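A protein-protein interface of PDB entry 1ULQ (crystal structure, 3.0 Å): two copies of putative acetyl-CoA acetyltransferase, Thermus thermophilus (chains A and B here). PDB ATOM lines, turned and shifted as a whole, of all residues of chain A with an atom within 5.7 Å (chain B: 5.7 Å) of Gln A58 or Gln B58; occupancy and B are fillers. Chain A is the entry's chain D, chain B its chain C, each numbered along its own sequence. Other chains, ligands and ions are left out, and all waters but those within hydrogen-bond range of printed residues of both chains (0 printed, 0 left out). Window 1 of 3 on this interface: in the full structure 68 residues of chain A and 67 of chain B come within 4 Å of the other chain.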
ATOM      1  N   CYS A  55      22.517 -13.496 -16.365  1.00  0.00           N
ATOM      2  CA  CYS A  55      21.479 -14.255 -17.059  1.00  0.00           C
ATOM      3  C   CYS A  55      22.136 -15.452 -17.726  1.00  0.00           C
ATOM      4  O   CYS A  55      22.938 -15.291 -18.649  1.00  0.00           O
ATOM      5  CB  CYS A  55      20.788 -13.376 -18.103  1.00  0.00           C
ATOM      6  SG  CYS A  55      19.561 -14.229 -19.118  1.00  0.00           S
ATOM      7  N   ALA A  56      21.782 -16.647 -17.262  1.00  0.00           N
ATOM      8  CA  ALA A  56      22.354 -17.897 -17.761  1.00  0.00           C
ATOM      9  C   ALA A  56      22.032 -18.262 -19.208  1.00  0.00           C
ATOM     10  O   ALA A  56      22.847 -18.891 -19.886  1.00  0.00           O
ATOM     11  CB  ALA A  56      21.941 -19.030 -16.850  1.00  0.00           C
ATOM     12  N   ASN A  57      20.858 -17.860 -19.682  1.00  0.00           N
ATOM     13  CA  ASN A  57      20.399 -18.183 -21.034  1.00  0.00           C
ATOM     14  C   ASN A  57      19.846 -16.942 -21.721  1.00  0.00           C
ATOM     15  O   ASN A  57      18.718 -16.535 -21.432  1.00  0.00           O
ATOM     16  CB  ASN A  57      19.298 -19.248 -20.917  1.00  0.00           C
ATOM     17  CG  ASN A  57      18.433 -19.370 -22.164  1.00  0.00           C
ATOM     18  OD1 ASN A  57      17.316 -19.876 -22.090  1.00  0.00           O
ATOM     19  ND2 ASN A  57      18.944 -18.928 -23.305  1.00  0.00           N
ATOM     20  N   GLN A  58      20.598 -16.345 -22.638  1.00  0.00           N
ATOM     21  CA  GLN A  58      20.095 -15.139 -23.294  1.00  0.00           C
ATOM     22  C   GLN A  58      19.570 -15.374 -24.709  1.00  0.00           C
ATOM     23  O   GLN A  58      19.753 -14.536 -25.606  1.00  0.00           O
ATOM     24  CB  GLN A  58      21.186 -14.083 -23.316  1.00  0.00           C
ATOM     25  CG  GLN A  58      21.671 -13.704 -21.948  1.00  0.00           C
ATOM     26  CD  GLN A  58      23.091 -13.224 -21.977  1.00  0.00           C
ATOM     27  OE1 GLN A  58      23.445 -12.359 -22.783  1.00  0.00           O
ATOM     28  NE2 GLN A  58      23.923 -13.779 -21.102  1.00  0.00           N
ATOM     29  N   ALA A  59      18.884 -16.502 -24.881  1.00  0.00           N
ATOM     30  CA  ALA A  59      18.343 -16.906 -26.170  1.00  0.00           C
ATOM     31  C   ALA A  59      16.905 -16.488 -26.482  1.00  0.00           C
ATOM     32  O   ALA A  59      16.502 -16.479 -27.643  1.00  0.00           O
ATOM     33  CB  ALA A  59      18.470 -18.401 -26.303  1.00  0.00           C
ATOM     34  N   GLY A  60      16.139 -16.133 -25.459  1.00  0.00           N
ATOM     35  CA  GLY A  60      14.756 -15.757 -25.682  1.00  0.00           C
ATOM     36  C   GLY A  60      14.441 -14.292 -25.494  1.00  0.00           C
ATOM     37  O   GLY A  60      15.119 -13.429 -26.040  1.00  0.00           O
ATOM     38  N   ASP A  62      15.107 -12.605 -23.343  1.00  0.00           N
ATOM     39  CA  ASP A  62      16.239 -12.006 -22.637  1.00  0.00           C
ATOM     40  C   ASP A  62      17.453 -11.870 -23.560  1.00  0.00           C
ATOM     41  O   ASP A  62      18.597 -11.778 -23.098  1.00  0.00           O
ATOM     42  CB  ASP A  62      16.624 -12.866 -21.423  1.00  0.00           C
ATOM     43  CG  ASP A  62      16.711 -14.349 -21.761  1.00  0.00           C
ATOM     44  OD1 ASP A  62      17.052 -14.677 -22.915  1.00  0.00           O
ATOM     45  OD2 ASP A  62      16.447 -15.194 -20.875  1.00  0.00           O
ATOM     46  N   ASN A  63      17.196 -11.845 -24.864  1.00  0.00           N
ATOM     47  CA  ASN A  63      18.264 -11.761 -25.843  1.00  0.00           C
ATOM     48  C   ASN A  63      18.803 -10.366 -26.023  1.00  0.00           C
ATOM     49  O   ASN A  63      18.152  -9.377 -25.685  1.00  0.00           O
ATOM     50  CB  ASN A  63      17.787 -12.306 -27.204  1.00  0.00           C
ATOM     51  CG  ASN A  63      16.944 -11.294 -28.004  1.00  0.00           C
ATOM     52  OD1 ASN A  63      17.475 -10.406 -28.676  1.00  0.00           O
ATOM     53  ND2 ASN A  63      15.631 -11.433 -27.931  1.00  0.00           N
ATOM     54  N   ARG A  64      20.010 -10.310 -26.563  1.00  0.00           N
ATOM     55  CA  ARG A  64      20.686  -9.061 -26.855  1.00  0.00           C
ATOM     56  C   ARG A  64      20.832  -8.076 -25.713  1.00  0.00           C
ATOM     57  O   ARG A  64      20.397  -6.922 -25.822  1.00  0.00           O
ATOM     58  CB  ARG A  64      20.014  -8.367 -28.037  1.00  0.00           C
ATOM     59  CG  ARG A  64      19.978  -9.207 -29.304  1.00  0.00           C
ATOM     60  CD  ARG A  64      20.366  -8.367 -30.498  1.00  0.00           C
ATOM     61  NE  ARG A  64      19.495  -7.208 -30.613  1.00  0.00           N
ATOM     62  CZ  ARG A  64      19.812  -6.105 -31.274  1.00  0.00           C
ATOM     63  NH1 ARG A  64      20.983  -6.006 -31.888  1.00  0.00           N
ATOM     64  NH2 ARG A  64      18.962  -5.090 -31.298  1.00  0.00           N
ATOM     65  N   ASN A  65      21.442  -8.553 -24.624  1.00  0.00           N
ATOM     66  CA  ASN A  65      21.760  -7.742 -23.444  1.00  0.00           C
ATOM     67  C   ASN A  65      20.568  -7.267 -22.621  1.00  0.00           C
ATOM     68  O   ASN A  65      20.169  -6.100 -22.674  1.00  0.00           O
ATOM     69  CB  ASN A  65      22.636  -6.554 -23.891  1.00  0.00           C
ATOM     70  CG  ASN A  65      23.237  -5.797 -22.733  1.00  0.00           C
ATOM     71  OD1 ASN A  65      23.663  -6.384 -21.747  1.00  0.00           O
ATOM     72  ND2 ASN A  65      23.296  -4.477 -22.861  1.00  0.00           N
ATOM     73  N   VAL A  66      20.024  -8.186 -21.836  1.00  0.00           N
ATOM     74  CA  VAL A  66      18.874  -7.890 -20.995  1.00  0.00           C
ATOM     75  C   VAL A  66      19.050  -6.651 -20.123  1.00  0.00           C
ATOM     76  O   VAL A  66      18.101  -5.884 -19.931  1.00  0.00           O
ATOM     77  CB  VAL A  66      18.542  -9.067 -20.074  1.00  0.00           C
ATOM     78  CG1 VAL A  66      17.093  -9.432 -20.227  1.00  0.00           C
ATOM     79  CG2 VAL A  66      19.408 -10.246 -20.416  1.00  0.00           C
ATOM     80  N   THR A  84      25.286  -7.543 -19.729  1.00  0.00           N
ATOM     81  CA  THR A  84      24.834  -8.808 -19.169  1.00  0.00           C
ATOM     82  C   THR A  84      26.016  -9.763 -19.024  1.00  0.00           C
ATOM     83  O   THR A  84      26.681 -10.101 -19.998  1.00  0.00           O
ATOM     84  CB  THR A  84      23.743  -9.484 -20.078  1.00  0.00           C
ATOM     85  OG1 THR A  84      22.554  -8.685 -20.095  1.00  0.00           O
ATOM     86  CG2 THR A  84      23.384 -10.879 -19.563  1.00  0.00           C
ATOM     87  N   VAL A  85      26.275 -10.196 -17.796  1.00  0.00           N
ATOM     88  CA  VAL A  85      27.357 -11.127 -17.524  1.00  0.00           C
ATOM     89  C   VAL A  85      26.781 -12.524 -17.396  1.00  0.00           C
ATOM     90  O   VAL A  85      25.657 -12.686 -16.950  1.00  0.00           O
ATOM     91  CB  VAL A  85      28.065 -10.767 -16.231  1.00  0.00           C
ATOM     92  CG1 VAL A  85      28.858  -9.477 -16.429  1.00  0.00           C
ATOM     93  CG2 VAL A  85      27.050 -10.622 -15.113  1.00  0.00           C
ATOM     94  N   ASN A  86      27.553 -13.532 -17.780  1.00  0.00           N
ATOM     95  CA  ASN A  86      27.088 -14.916 -17.719  1.00  0.00           C
ATOM     96  C   ASN A  86      28.140 -15.899 -17.212  1.00  0.00           C
ATOM     97  O   ASN A  86      29.048 -16.283 -17.947  1.00  0.00           O
ATOM     98  CB  ASN A  86      26.610 -15.360 -19.109  1.00  0.00           C
ATOM     99  CG  ASN A  86      26.309 -16.858 -19.189  1.00  0.00           C
ATOM    100  OD1 ASN A  86      25.412 -17.367 -18.525  1.00  0.00           O
ATOM    101  ND2 ASN A  86      27.063 -17.566 -20.013  1.00  0.00           N
ATOM    102  N   ARG A 148      23.535 -28.848 -24.430  1.00  0.00           N
ATOM    103  CA  ARG A 148      22.917 -28.770 -25.745  1.00  0.00           C
ATOM    104  C   ARG A 148      23.990 -28.400 -26.759  1.00  0.00           C
ATOM    105  O   ARG A 148      25.037 -27.867 -26.385  1.00  0.00           O
ATOM    106  CB  ARG A 148      21.794 -27.735 -25.720  1.00  0.00           C
ATOM    107  CG  ARG A 148      22.101 -26.477 -24.936  1.00  0.00           C
ATOM    108  CD  ARG A 148      20.815 -25.839 -24.453  1.00  0.00           C
ATOM    109  NE  ARG A 148      20.857 -24.379 -24.479  1.00  0.00           N
ATOM    110  CZ  ARG A 148      20.908 -23.606 -23.399  1.00  0.00           C
ATOM    111  NH1 ARG A 148      20.927 -24.155 -22.188  1.00  0.00           N
ATOM    112  NH2 ARG A 148      20.931 -22.280 -23.534  1.00  0.00           N
ATOM    113  N   CYS B  55      30.480 -12.256 -26.065  1.00  0.00           N
ATOM    114  CA  CYS B  55      29.695 -12.981 -27.049  1.00  0.00           C
ATOM    115  C   CYS B  55      28.285 -12.385 -27.113  1.00  0.00           C
ATOM    116  O   CYS B  55      27.545 -12.404 -26.130  1.00  0.00           O
ATOM    117  CB  CYS B  55      29.636 -14.451 -26.665  1.00  0.00           C
ATOM    118  SG  CYS B  55      28.978 -15.489 -27.954  1.00  0.00           S
ATOM    119  N   ALA B  56      27.921 -11.871 -28.284  1.00  0.00           N
ATOM    120  CA  ALA B  56      26.635 -11.221 -28.494  1.00  0.00           C
ATOM    121  C   ALA B  56      25.425 -12.129 -28.550  1.00  0.00           C
ATOM    122  O   ALA B  56      24.296 -11.685 -28.317  1.00  0.00           O
ATOM    123  CB  ALA B  56      26.691 -10.385 -29.760  1.00  0.00           C
ATOM    124  N   ASN B  57      25.644 -13.394 -28.867  1.00  0.00           N
ATOM    125  CA  ASN B  57      24.536 -14.338 -28.967  1.00  0.00           C
ATOM    126  C   ASN B  57      24.982 -15.665 -28.396  1.00  0.00           C
ATOM    127  O   ASN B  57      25.737 -16.388 -29.039  1.00  0.00           O
ATOM    128  CB  ASN B  57      24.151 -14.494 -30.442  1.00  0.00           C
ATOM    129  CG  ASN B  57      23.639 -15.879 -30.780  1.00  0.00           C
ATOM    130  OD1 ASN B  57      23.826 -16.352 -31.897  1.00  0.00           O
ATOM    131  ND2 ASN B  57      22.983 -16.527 -29.827  1.00  0.00           N
ATOM    132  N   GLN B  58      24.518 -16.015 -27.209  1.00  0.00           N
ATOM    133  CA  GLN B  58      24.969 -17.268 -26.645  1.00  0.00           C
ATOM    134  C   GLN B  58      23.926 -18.359 -26.674  1.00  0.00           C
ATOM    135  O   GLN B  58      23.826 -19.142 -25.740  1.00  0.00           O
ATOM    136  CB  GLN B  58      25.446 -17.020 -25.226  1.00  0.00           C
ATOM    137  CG  GLN B  58      26.592 -16.041 -25.166  1.00  0.00           C
ATOM    138  CD  GLN B  58      26.661 -15.350 -23.833  1.00  0.00           C
ATOM    139  OE1 GLN B  58      26.475 -15.981 -22.803  1.00  0.00           O
ATOM    140  NE2 GLN B  58      26.932 -14.047 -23.841  1.00  0.00           N
ATOM    141  N   ALA B  59      23.179 -18.436 -27.769  1.00  0.00           N
ATOM    142  CA  ALA B  59      22.108 -19.421 -27.904  1.00  0.00           C
ATOM    143  C   ALA B  59      22.479 -20.759 -28.561  1.00  0.00           C
ATOM    144  O   ALA B  59      21.822 -21.776 -28.316  1.00  0.00           O
ATOM    145  CB  ALA B  59      20.937 -18.786 -28.648  1.00  0.00           C
ATOM    146  N   GLY B  60      23.534 -20.768 -29.372  1.00  0.00           N
ATOM    147  CA  GLY B  60      23.930 -21.991 -30.055  1.00  0.00           C
ATOM    148  C   GLY B  60      25.098 -22.766 -29.474  1.00  0.00           C
ATOM    149  O   GLY B  60      25.129 -23.073 -28.289  1.00  0.00           O
ATOM    150  N   ASP B  62      27.647 -21.769 -28.698  1.00  0.00           N
ATOM    151  CA  ASP B  62      28.340 -20.887 -27.768  1.00  0.00           C
ATOM    152  C   ASP B  62      27.536 -20.724 -26.481  1.00  0.00           C
ATOM    153  O   ASP B  62      27.728 -19.764 -25.736  1.00  0.00           O
ATOM    154  CB  ASP B  62      28.550 -19.517 -28.403  1.00  0.00           C
ATOM    155  CG  ASP B  62      27.294 -18.990 -29.084  1.00  0.00           C
ATOM    156  OD1 ASP B  62      26.177 -19.297 -28.612  1.00  0.00           O
ATOM    157  OD2 ASP B  62      27.426 -18.252 -30.086  1.00  0.00           O
ATOM    158  N   ASN B  63      26.643 -21.672 -26.216  1.00  0.00           N
ATOM    159  CA  ASN B  63      25.790 -21.613 -25.034  1.00  0.00           C
ATOM    160  C   ASN B  63      26.443 -22.002 -23.697  1.00  0.00           C
ATOM    161  O   ASN B  63      27.454 -22.709 -23.641  1.00  0.00           O
ATOM    162  CB  ASN B  63      24.549 -22.491 -25.249  1.00  0.00           C
ATOM    163  CG  ASN B  63      24.816 -23.969 -24.973  1.00  0.00           C
ATOM    164  OD1 ASN B  63      24.885 -24.399 -23.814  1.00  0.00           O
ATOM    165  ND2 ASN B  63      24.979 -24.753 -26.041  1.00  0.00           N
ATOM    166  N   ARG B  64      25.824 -21.530 -22.623  1.00  0.00           N
ATOM    167  CA  ARG B  64      26.255 -21.805 -21.263  1.00  0.00           C
ATOM    168  C   ARG B  64      27.693 -21.436 -20.932  1.00  0.00           C
ATOM    169  O   ARG B  64      28.483 -22.277 -20.466  1.00  0.00           O
ATOM    170  CB  ARG B  64      25.976 -23.273 -20.905  1.00  0.00           C
ATOM    171  CG  ARG B  64      24.474 -23.648 -20.966  1.00  0.00           C
ATOM    172  CD  ARG B  64      24.112 -24.744 -19.983  1.00  0.00           C
ATOM    173  NE  ARG B  64      24.997 -25.884 -20.152  1.00  0.00           N
ATOM    174  CZ  ARG B  64      25.453 -26.631 -19.153  1.00  0.00           C
ATOM    175  NH1 ARG B  64      25.103 -26.361 -17.901  1.00  0.00           N
ATOM    176  NH2 ARG B  64      26.274 -27.642 -19.405  1.00  0.00           N
ATOM    177  N   ASN B  65      28.012 -20.162 -21.180  1.00  0.00           N
ATOM    178  CA  ASN B  65      29.320 -19.599 -20.881  1.00  0.00           C
ATOM    179  C   ASN B  65      30.444 -20.159 -21.739  1.00  0.00           C
ATOM    180  O   ASN B  65      31.161 -21.066 -21.323  1.00  0.00           O
ATOM    181  CB  ASN B  65      29.620 -19.825 -19.397  1.00  0.00           C
ATOM    182  CG  ASN B  65      30.854 -19.100 -18.931  1.00  0.00           C
ATOM    183  OD1 ASN B  65      31.114 -17.972 -19.345  1.00  0.00           O
ATOM    184  ND2 ASN B  65      31.615 -19.734 -18.042  1.00  0.00           N
ATOM    185  N   VAL B  66      30.601 -19.604 -22.936  1.00  0.00           N
ATOM    186  CA  VAL B  66      31.641 -20.056 -23.857  1.00  0.00           C
ATOM    187  C   VAL B  66      33.026 -19.969 -23.246  1.00  0.00           C
ATOM    188  O   VAL B  66      33.860 -20.848 -23.457  1.00  0.00           O
ATOM    189  CB  VAL B  66      31.690 -19.210 -25.133  1.00  0.00           C
ATOM    190  CG1 VAL B  66      31.873 -20.118 -26.340  1.00  0.00           C
ATOM    191  CG2 VAL B  66      30.455 -18.354 -25.237  1.00  0.00           C
ATOM    192  N   THR B  84      31.405 -15.194 -19.364  1.00  0.00           N
ATOM    193  CA  THR B  84      31.110 -14.612 -20.666  1.00  0.00           C
ATOM    194  C   THR B  84      30.335 -13.299 -20.517  1.00  0.00           C
ATOM    195  O   THR B  84      29.192 -13.282 -20.060  1.00  0.00           O
ATOM    196  CB  THR B  84      30.288 -15.584 -21.536  1.00  0.00           C
ATOM    197  OG1 THR B  84      31.057 -16.760 -21.809  1.00  0.00           O
ATOM    198  CG2 THR B  84      29.922 -14.937 -22.841  1.00  0.00           C
ATOM    199  N   VAL B  85      30.963 -12.198 -20.906  1.00  0.00           N
ATOM    200  CA  VAL B  85      30.327 -10.894 -20.822  1.00  0.00           C
ATOM    201  C   VAL B  85      29.585 -10.562 -22.116  1.00  0.00           C
ATOM    202  O   VAL B  85      29.983 -10.990 -23.199  1.00  0.00           O
ATOM    203  CB  VAL B  85      31.371  -9.799 -20.537  1.00  0.00           C
ATOM    204  CG1 VAL B  85      31.855  -9.923 -19.098  1.00  0.00           C
ATOM    205  CG2 VAL B  85      32.542  -9.915 -21.505  1.00  0.00           C
ATOM    206  N   ASN B  86      28.504  -9.798 -22.006  1.00  0.00           N
ATOM    207  CA  ASN B  86      27.729  -9.434 -23.183  1.00  0.00           C
ATOM    208  C   ASN B  86      27.179  -8.021 -23.187  1.00  0.00           C
ATOM    209  O   ASN B  86      26.184  -7.740 -22.525  1.00  0.00           O
ATOM    210  CB  ASN B  86      26.568 -10.403 -23.374  1.00  0.00           C
ATOM    211  CG  ASN B  86      25.603  -9.939 -24.442  1.00  0.00           C
ATOM    212  OD1 ASN B  86      25.987  -9.218 -25.367  1.00  0.00           O
ATOM    213  ND2 ASN B  86      24.344 -10.359 -24.332  1.00  0.00           N
ATOM    214  N   ARG B 148      14.463  -9.489 -31.909  1.00  0.00           N
ATOM    215  CA  ARG B 148      13.670 -10.707 -31.872  1.00  0.00           C
ATOM    216  C   ARG B 148      12.948 -10.779 -30.533  1.00  0.00           C
ATOM    217  O   ARG B 148      13.333 -10.087 -29.591  1.00  0.00           O
ATOM    218  CB  ARG B 148      14.567 -11.932 -32.102  1.00  0.00           C
ATOM    219  CG  ARG B 148      15.974 -11.873 -31.496  1.00  0.00           C
ATOM    220  CD  ARG B 148      16.852 -13.029 -32.039  1.00  0.00           C
ATOM    221  NE  ARG B 148      18.023 -13.335 -31.209  1.00  0.00           N
ATOM    222  CZ  ARG B 148      19.176 -12.673 -31.247  1.00  0.00           C
ATOM    223  NH1 ARG B 148      19.333 -11.655 -32.082  1.00  0.00           N
ATOM    224  NH2 ARG B 148      20.175 -13.024 -30.441  1.00  0.00           N
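The side-chain amide oxygen (OE1) of Gln B58 lies within hydrogen-bond range of the side-chain amide nitrogen (ND2) of Asn A86, at 3.3 Å.
The backbone carbonyl oxygen (O) of Arg A148 sits at hydrogen-bond distance from the side-chain amide nitrogen (ND2) of Asn B63 (3.1 Å).
The backbone NH (N) of Asn B65 lies close to the side-chain amide nitrogen (ND2) of Asn A86 (3.0 Å).
The backbone carbonyl oxygen (O) of Thr B84 is in hydrogen-bond range of the backbone NH (N) of Asn A86 (2.8 Å).
The side-chain amide nitrogen of Asn B86 sits at hydrogen-bond distance from the side-chain amide oxygen of Gln A58 (2.7 Å).
The backbone carbonyl oxygen of Asn B86 sits close to the side-chain amide oxygen of Asn A65 (3.0 Å).
The backbone NH (N) of Asn B86 is in hydrogen-bond range of the backbone carbonyl oxygen (O) of Thr A84, 2.7 Å away.
The side-chain amide nitrogen (ND2) of Asn A63 sits at hydrogen-bond distance from the backbone carbonyl oxygen (O) of Arg B148 (3.1 Å).
The backbone carbonyl oxygen (O) of Cys B55 sits at hydrogen-bond distance from the side-chain amide nitrogen (NE2) of Gln B58 (2.9 Å).
The side-chain amide nitrogen of Asn B57 lies close to the backbone NH of Ala B59 (2.8 Å).
The backbone NH (N) of Ala B59 is in hydrogen-bond range of the side-chain carboxylate (OD1) of Asp B62 (3.2 Å).
The side-chain amide nitrogen (ND2) of Asn B63 is in hydrogen-bond range of the backbone carbonyl oxygen (O) of Gly B60, at 2.8 Å.
OD1 of Asp A62 lies within hydrogen-bond range of N of Ala A59.
The side-chain amide nitrogen (ND2) of Asn A63 sits at hydrogen-bond distance from the backbone carbonyl oxygen (O) of Gly A60, at 2.8 Å.
Among the printed residues, merely in contact across the chains: Gln A58 with Gln B58 (3.8 Å), Ala A59 with Ala B59 (3.4 Å), Arg A64 with Arg B148 (3.8 Å), Thr A84 with Val B85 (3.6 Å), Val A85 with Thr B84 (3.7 Å) and Arg A148 with Arg B64 (3.8 Å).
Gln A58 touches just these residues of chain B: Gln B58 and Asn B86.
Gly A60 touches none of the printed residues of chain B.
Of the printed residues of chain B, Thr A84 touches Val B85 and Asn B86.
Of the printed residues of chain B, Asn A86 touches Gln B58, Asn B65 and Thr B84.
Gln B58 touches just these residues of chain A: Gln A58 (3.8 Å) and Asn A86 (3.3 Å).
Of the printed residues of chain A, Arg B64 touches Arg A148 (3.8 Å).
Val B66 touches none of the printed residues of chain A.
Printed residues of chain A within 4 Å of Val B85: Thr A84 (3.6 Å).
The nearest residue of chain A that does not touch Gln B58 is Arg A148 (4.8 Å).
The nearest printed residue of chain B that does not touch Asn A63 is Asn B86 (5.8 Å).
Of the 15 printed residues of chain B, 9 touch a printed residue of chain A.
Printed residues of chain B that touch a printed residue of chain A: Gln B58, Ala B59, Asn B63, Arg B64, Asn B65, Thr B84, Val B85, Asn B86 and Arg B148.
Hydrophobic or aromatic side chains of chain B within 4 Å of the printed part of chain A: Ala B59.
Along chain A the printed residues that touch a printed residue of chain B span positions 58 to 148.
Among the printed residues, 14 pairs touch across the chains.
Among the printed residues, no Asp or Glu carboxylate lies within 4 Å of a Lys or Arg side-chain nitrogen of the other chain.
Gln A58 touches its own counterpart, Gln B58.
Asn A63 touches Arg B148, and with the chains exchanged Arg A148 touches Asn B63.
Asn A65 touches Asn B86, and with the chains exchanged Asn A86 touches Asn B65.
Thr A84 touches Val B85, and with the chains exchanged Val A85 touches Thr B84.
15 positions are printed for both chains.
Of the 14 pairs that touch across the chains among the printed residues, 14 have their exchanged pair printed and touching as well.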
